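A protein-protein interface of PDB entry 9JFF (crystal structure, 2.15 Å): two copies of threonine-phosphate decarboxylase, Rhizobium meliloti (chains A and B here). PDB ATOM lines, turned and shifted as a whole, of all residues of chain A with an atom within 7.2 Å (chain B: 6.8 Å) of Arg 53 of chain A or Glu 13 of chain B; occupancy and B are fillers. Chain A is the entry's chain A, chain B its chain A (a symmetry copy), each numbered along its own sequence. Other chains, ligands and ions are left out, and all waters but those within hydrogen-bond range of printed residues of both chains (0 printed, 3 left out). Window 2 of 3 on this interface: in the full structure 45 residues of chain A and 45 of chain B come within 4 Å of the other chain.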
ATOM      1  N   LEU A  50      -2.958   6.654 -19.901  1.00  0.00           N
ATOM      2  CA  LEU A  50      -3.912   5.935 -20.732  1.00  0.00           C
ATOM      3  C   LEU A  50      -4.209   6.762 -21.981  1.00  0.00           C
ATOM      4  O   LEU A  50      -4.337   7.991 -21.889  1.00  0.00           O
ATOM      5  CB  LEU A  50      -5.202   5.667 -19.950  1.00  0.00           C
ATOM      6  CG  LEU A  50      -5.114   4.621 -18.839  1.00  0.00           C
ATOM      7  CD1 LEU A  50      -6.348   4.676 -17.950  1.00  0.00           C
ATOM      8  CD2 LEU A  50      -4.932   3.213 -19.431  1.00  0.00           C
ATOM      9  N   PRO A  51      -4.296   6.140 -23.161  1.00  0.00           N
ATOM     10  CA  PRO A  51      -4.396   6.927 -24.404  1.00  0.00           C
ATOM     11  C   PRO A  51      -5.602   7.851 -24.375  1.00  0.00           C
ATOM     12  O   PRO A  51      -6.735   7.422 -24.148  1.00  0.00           O
ATOM     13  CB  PRO A  51      -4.508   5.857 -25.503  1.00  0.00           C
ATOM     14  CG  PRO A  51      -4.759   4.566 -24.795  1.00  0.00           C
ATOM     15  CD  PRO A  51      -4.172   4.699 -23.425  1.00  0.00           C
ATOM     16  N   ASP A  52      -5.336   9.139 -24.578  1.00  0.00           N
ATOM     17  CA  ASP A  52      -6.332  10.192 -24.463  1.00  0.00           C
ATOM     18  C   ASP A  52      -7.123  10.329 -25.757  1.00  0.00           C
ATOM     19  O   ASP A  52      -6.638  10.013 -26.847  1.00  0.00           O
ATOM     20  CB  ASP A  52      -5.657  11.527 -24.139  1.00  0.00           C
ATOM     21  CG  ASP A  52      -5.081  11.575 -22.726  1.00  0.00           C
ATOM     22  OD1 ASP A  52      -5.862  11.503 -21.752  1.00  0.00           O
ATOM     23  OD2 ASP A  52      -3.844  11.678 -22.592  1.00  0.00           O
ATOM     24  N   ARG A  53      -8.352  10.837 -25.628  1.00  0.00           N
ATOM     25  CA  ARG A  53      -9.183  11.067 -26.806  1.00  0.00           C
ATOM     26  C   ARG A  53      -8.467  11.946 -27.824  1.00  0.00           C
ATOM     27  O   ARG A  53      -8.594  11.742 -29.036  1.00  0.00           O
ATOM     28  CB  ARG A  53     -10.513  11.702 -26.395  1.00  0.00           C
ATOM     29  CG  ARG A  53     -11.525  11.819 -27.532  1.00  0.00           C
ATOM     30  CD  ARG A  53     -12.672  12.765 -27.178  1.00  0.00           C
ATOM     31  NE  ARG A  53     -12.362  14.157 -27.490  1.00  0.00           N
ATOM     32  CZ  ARG A  53     -13.133  15.188 -27.167  1.00  0.00           C
ATOM     33  NH1 ARG A  53     -14.264  15.024 -26.502  1.00  0.00           N
ATOM     34  NH2 ARG A  53     -12.757  16.416 -27.517  1.00  0.00           N
ATOM     35  N   GLN A  54      -7.706  12.935 -27.350  1.00  0.00           N
ATOM     36  CA  GLN A  54      -6.995  13.818 -28.270  1.00  0.00           C
ATOM     37  C   GLN A  54      -5.925  13.061 -29.052  1.00  0.00           C
ATOM     38  O   GLN A  54      -5.711  13.328 -30.241  1.00  0.00           O
ATOM     39  CB  GLN A  54      -6.374  14.985 -27.505  1.00  0.00           C
ATOM     40  CG  GLN A  54      -5.803  16.064 -28.417  1.00  0.00           C
ATOM     41  CD  GLN A  54      -6.880  16.728 -29.260  1.00  0.00           C
ATOM     42  OE1 GLN A  54      -7.835  17.301 -28.731  1.00  0.00           O
ATOM     43  NE2 GLN A  54      -6.738  16.647 -30.577  1.00  0.00           N
ATOM     44  N   THR A  55      -5.239  12.121 -28.395  1.00  0.00           N
ATOM     45  CA  THR A  55      -4.239  11.298 -29.070  1.00  0.00           C
ATOM     46  C   THR A  55      -4.886  10.413 -30.128  1.00  0.00           C
ATOM     47  O   THR A  55      -4.356  10.260 -31.237  1.00  0.00           O
ATOM     48  CB  THR A  55      -3.498  10.451 -28.035  1.00  0.00           C
ATOM     49  OG1 THR A  55      -3.081  11.288 -26.950  1.00  0.00           O
ATOM     50  CG2 THR A  55      -2.279   9.775 -28.646  1.00  0.00           C
ATOM     51  N   VAL A  56      -6.039   9.830 -29.800  1.00  0.00           N
ATOM     52  CA  VAL A  56      -6.793   9.042 -30.771  1.00  0.00           C
ATOM     53  C   VAL A  56      -7.220   9.916 -31.948  1.00  0.00           C
ATOM     54  O   VAL A  56      -6.995   9.572 -33.118  1.00  0.00           O
ATOM     55  CB  VAL A  56      -8.003   8.386 -30.083  1.00  0.00           C
ATOM     56  CG1 VAL A  56      -8.858   7.623 -31.089  1.00  0.00           C
ATOM     57  CG2 VAL A  56      -7.537   7.489 -28.932  1.00  0.00           C
ATOM     58  N   ASP A  57      -7.839  11.064 -31.654  1.00  0.00           N
ATOM     59  CA  ASP A  57      -8.420  11.890 -32.711  1.00  0.00           C
ATOM     60  C   ASP A  57      -7.362  12.379 -33.688  1.00  0.00           C
ATOM     61  O   ASP A  57      -7.614  12.447 -34.896  1.00  0.00           O
ATOM     62  CB  ASP A  57      -9.161  13.080 -32.109  1.00  0.00           C
ATOM     63  CG  ASP A  57     -10.467  12.682 -31.449  1.00  0.00           C
ATOM     64  OD1 ASP A  57     -10.974  11.575 -31.731  1.00  0.00           O
ATOM     65  OD2 ASP A  57     -10.986  13.488 -30.650  1.00  0.00           O
ATOM     66  N   ASP A  58      -6.173  12.738 -33.187  1.00  0.00           N
ATOM     67  CA  ASP A  58      -5.112  13.200 -34.074  1.00  0.00           C
ATOM     68  C   ASP A  58      -4.647  12.084 -34.998  1.00  0.00           C
ATOM     69  O   ASP A  58      -4.360  12.327 -36.175  1.00  0.00           O
ATOM     70  CB  ASP A  58      -3.931  13.741 -33.270  1.00  0.00           C
ATOM     71  CG  ASP A  58      -4.255  15.034 -32.540  1.00  0.00           C
ATOM     72  OD1 ASP A  58      -5.279  15.678 -32.870  1.00  0.00           O
ATOM     73  OD2 ASP A  58      -3.480  15.407 -31.632  1.00  0.00           O
ATOM     74  N   ALA A  59      -4.554  10.855 -34.482  1.00  0.00           N
ATOM     75  CA  ALA A  59      -4.200   9.729 -35.343  1.00  0.00           C
ATOM     76  C   ALA A  59      -5.286   9.474 -36.381  1.00  0.00           C
ATOM     77  O   ALA A  59      -4.985   9.140 -37.534  1.00  0.00           O
ATOM     78  CB  ALA A  59      -3.948   8.473 -34.506  1.00  0.00           C
ATOM     79  N   ARG A  60      -6.556   9.633 -35.993  1.00  0.00           N
ATOM     80  CA  ARG A  60      -7.647   9.417 -36.942  1.00  0.00           C
ATOM     81  C   ARG A  60      -7.634  10.466 -38.045  1.00  0.00           C
ATOM     82  O   ARG A  60      -7.868  10.142 -39.217  1.00  0.00           O
ATOM     83  CB  ARG A  60      -9.004   9.428 -36.230  1.00  0.00           C
ATOM     84  CG  ARG A  60      -9.162   8.375 -35.145  1.00  0.00           C
ATOM     85  CD  ARG A  60     -10.590   8.341 -34.599  1.00  0.00           C
ATOM     86  NE  ARG A  60     -11.518   7.732 -35.543  1.00  0.00           N
ATOM     87  CZ  ARG A  60     -12.790   7.472 -35.277  1.00  0.00           C
ATOM     88  NH1 ARG A  60     -13.329   7.789 -34.109  1.00  0.00           N
ATOM     89  NH2 ARG A  60     -13.540   6.878 -36.203  1.00  0.00           N
ATOM     90  N   VAL B   6     -17.788   6.459 -18.426  1.00  0.00           N
ATOM     91  CA  VAL B   6     -16.846   7.577 -18.339  1.00  0.00           C
ATOM     92  C   VAL B   6     -15.803   7.188 -17.294  1.00  0.00           C
ATOM     93  O   VAL B   6     -15.956   7.438 -16.098  1.00  0.00           O
ATOM     94  CB  VAL B   6     -17.540   8.897 -18.010  1.00  0.00           C
ATOM     95  CG1 VAL B   6     -16.516  10.037 -17.986  1.00  0.00           C
ATOM     96  CG2 VAL B   6     -18.636   9.190 -19.027  1.00  0.00           C
ATOM     97  N   GLY B   9      -9.294   9.614 -16.342  1.00  0.00           N
ATOM     98  CA  GLY B   9      -8.334   9.949 -17.373  1.00  0.00           C
ATOM     99  C   GLY B   9      -8.846  10.873 -18.458  1.00  0.00           C
ATOM    100  O   GLY B   9      -8.084  11.201 -19.377  1.00  0.00           O
ATOM    101  N   GLY B  10     -10.100  11.313 -18.382  1.00  0.00           N
ATOM    102  CA  GLY B  10     -10.696  12.098 -19.448  1.00  0.00           C
ATOM    103  C   GLY B  10     -10.285  13.558 -19.457  1.00  0.00           C
ATOM    104  O   GLY B  10     -11.142  14.450 -19.401  1.00  0.00           O
ATOM    105  N   ILE B  11      -8.975  13.811 -19.546  1.00  0.00           N
ATOM    106  CA  ILE B  11      -8.461  15.178 -19.539  1.00  0.00           C
ATOM    107  C   ILE B  11      -8.885  15.928 -20.795  1.00  0.00           C
ATOM    108  O   ILE B  11      -9.241  17.112 -20.731  1.00  0.00           O
ATOM    109  CB  ILE B  11      -6.931  15.173 -19.374  1.00  0.00           C
ATOM    110  CG1 ILE B  11      -6.562  14.803 -17.935  1.00  0.00           C
ATOM    111  CG2 ILE B  11      -6.349  16.527 -19.755  1.00  0.00           C
ATOM    112  CD1 ILE B  11      -6.959  15.863 -16.899  1.00  0.00           C
ATOM    113  N   THR B  12      -8.853  15.259 -21.956  1.00  0.00           N
ATOM    114  CA  THR B  12      -9.305  15.886 -23.194  1.00  0.00           C
ATOM    115  C   THR B  12     -10.703  16.464 -23.034  1.00  0.00           C
ATOM    116  O   THR B  12     -10.943  17.644 -23.311  1.00  0.00           O
ATOM    117  CB  THR B  12      -9.283  14.874 -24.347  1.00  0.00           C
ATOM    118  OG1 THR B  12      -7.941  14.428 -24.581  1.00  0.00           O
ATOM    119  CG2 THR B  12      -9.827  15.510 -25.625  1.00  0.00           C
ATOM    120  N   GLU B  13     -11.641  15.638 -22.575  1.00  0.00           N
ATOM    121  CA  GLU B  13     -13.014  16.091 -22.405  1.00  0.00           C
ATOM    122  C   GLU B  13     -13.139  17.112 -21.277  1.00  0.00           C
ATOM    123  O   GLU B  13     -13.948  18.040 -21.373  1.00  0.00           O
ATOM    124  CB  GLU B  13     -13.922  14.890 -22.144  1.00  0.00           C
ATOM    125  CG  GLU B  13     -13.898  13.825 -23.254  1.00  0.00           C
ATOM    126  CD  GLU B  13     -12.798  12.764 -23.086  1.00  0.00           C
ATOM    127  OE1 GLU B  13     -11.711  13.063 -22.534  1.00  0.00           O
ATOM    128  OE2 GLU B  13     -13.034  11.614 -23.518  1.00  0.00           O
ATOM    129  N   ALA B  14     -12.356  16.963 -20.204  1.00  0.00           N
ATOM    130  CA  ALA B  14     -12.435  17.922 -19.103  1.00  0.00           C
ATOM    131  C   ALA B  14     -11.964  19.302 -19.542  1.00  0.00           C
ATOM    132  O   ALA B  14     -12.623  20.312 -19.265  1.00  0.00           O
ATOM    133  CB  ALA B  14     -11.614  17.432 -17.911  1.00  0.00           C
ATOM    134  N   ALA B  15     -10.822  19.362 -20.233  1.00  0.00           N
ATOM    135  CA  ALA B  15     -10.280  20.640 -20.681  1.00  0.00           C
ATOM    136  C   ALA B  15     -11.219  21.329 -21.664  1.00  0.00           C
ATOM    137  O   ALA B  15     -11.351  22.558 -21.648  1.00  0.00           O
ATOM    138  CB  ALA B  15      -8.899  20.434 -21.309  1.00  0.00           C
ATOM    139  N   ALA B  16     -11.887  20.554 -22.527  1.00  0.00           N
ATOM    140  CA  ALA B  16     -12.817  21.156 -23.475  1.00  0.00           C
ATOM    141  C   ALA B  16     -14.008  21.786 -22.765  1.00  0.00           C
ATOM    142  O   ALA B  16     -14.574  22.771 -23.252  1.00  0.00           O
ATOM    143  CB  ALA B  16     -13.304  20.111 -24.482  1.00  0.00           C
ATOM    144  N   ARG B  17     -14.401  21.236 -21.622  1.00  0.00           N
ATOM    145  CA  ARG B  17     -15.560  21.735 -20.899  1.00  0.00           C
ATOM    146  C   ARG B  17     -15.195  22.847 -19.927  1.00  0.00           C
ATOM    147  O   ARG B  17     -15.963  23.801 -19.761  1.00  0.00           O
ATOM    148  CB  ARG B  17     -16.228  20.581 -20.159  1.00  0.00           C
ATOM    149  CG  ARG B  17     -17.439  20.951 -19.348  1.00  0.00           C
ATOM    150  CD  ARG B  17     -18.035  19.685 -18.766  1.00  0.00           C
ATOM    151  NE  ARG B  17     -19.194  19.943 -17.922  1.00  0.00           N
ATOM    152  CZ  ARG B  17     -19.875  18.998 -17.289  1.00  0.00           C
ATOM    153  NH1 ARG B  17     -19.540  17.719 -17.391  1.00  0.00           N
ATOM    154  NH2 ARG B  17     -20.915  19.342 -16.533  1.00  0.00           N
ATOM    155  N   TYR B  18     -14.024  22.759 -19.302  1.00  0.00           N
ATOM    156  CA  TYR B  18     -13.648  23.658 -18.222  1.00  0.00           C
ATOM    157  C   TYR B  18     -12.492  24.579 -18.576  1.00  0.00           C
ATOM    158  O   TYR B  18     -12.121  25.423 -17.752  1.00  0.00           O
ATOM    159  CB  TYR B  18     -13.293  22.851 -16.969  1.00  0.00           C
ATOM    160  CG  TYR B  18     -14.472  22.118 -16.354  1.00  0.00           C
ATOM    161  CD1 TYR B  18     -15.368  22.777 -15.522  1.00  0.00           C
ATOM    162  CD2 TYR B  18     -14.683  20.768 -16.600  1.00  0.00           C
ATOM    163  CE1 TYR B  18     -16.443  22.109 -14.955  1.00  0.00           C
ATOM    164  CE2 TYR B  18     -15.753  20.093 -16.036  1.00  0.00           C
ATOM    165  CZ  TYR B  18     -16.629  20.767 -15.213  1.00  0.00           C
ATOM    166  OH  TYR B  18     -17.692  20.095 -14.649  1.00  0.00           O
ATOM    167  N   TRP B  25      -3.474  20.768 -16.637  1.00  0.00           N
ATOM    168  CA  TRP B  25      -4.352  20.096 -15.695  1.00  0.00           C
ATOM    169  C   TRP B  25      -3.560  19.160 -14.791  1.00  0.00           C
ATOM    170  O   TRP B  25      -2.524  18.611 -15.174  1.00  0.00           O
ATOM    171  CB  TRP B  25      -5.418  19.296 -16.443  1.00  0.00           C
ATOM    172  CG  TRP B  25      -6.585  20.095 -16.899  1.00  0.00           C
ATOM    173  CD1 TRP B  25      -6.604  21.046 -17.884  1.00  0.00           C
ATOM    174  CD2 TRP B  25      -7.927  19.994 -16.409  1.00  0.00           C
ATOM    175  NE1 TRP B  25      -7.877  21.555 -18.021  1.00  0.00           N
ATOM    176  CE2 TRP B  25      -8.706  20.925 -17.128  1.00  0.00           C
ATOM    177  CE3 TRP B  25      -8.543  19.213 -15.424  1.00  0.00           C
ATOM    178  CZ2 TRP B  25     -10.071  21.094 -16.897  1.00  0.00           C
ATOM    179  CZ3 TRP B  25      -9.901  19.383 -15.194  1.00  0.00           C
ATOM    180  CH2 TRP B  25     -10.650  20.316 -15.928  1.00  0.00           C
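The side-chain carboxylate of Asp 52 of chain A lies close to the backbone carbonyl oxygen of Gly 9 of chain B, 3.3 Å away. The backbone NH (N) of Gln 54 of chain A lies within hydrogen-bond range of the side-chain hydroxyl (OG1) of Thr 12 of chain B.
OD1 of Asp 58 of chain A lies within hydrogen-bond range of NE2 of Gln 54 of chain A (2.9 Å). The side-chain carboxylate (OD2) of Asp 57 of chain A is in salt-bridge range of the guanidinium group (NE) of Arg 53 of chain A, 3.5 Å away.
Among the printed residues, pairs that only touch across the chains: Asp 52 of chain A with Thr 12 of chain B, Arg 53 of chain A with Thr 12 of chain B and Arg 53 of chain A with Glu 13 of chain B.
Of the printed residues of chain B, Asp 52 of chain A touches Gly 9 (3.3 Å) and Thr 12 (3.7 Å). Printed residues of chain B within 4 Å of Arg 53 of chain A: Thr 12 and Glu 13. Of the printed residues of chain B, Gln 54 of chain A touches Thr 12. Arg 60 of chain A touches none of the printed residues of chain B. Of the printed residues of chain A, Glu 13 of chain B touches Arg 53. The nearest printed residue of chain B that does not touch Arg 53 of chain A is Ala 16 of chain B (4.8 Å).
Printed residues of chain B that touch a printed residue of chain A: Gly 9, Thr 12 and Glu 13.
No position is printed for both chains.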
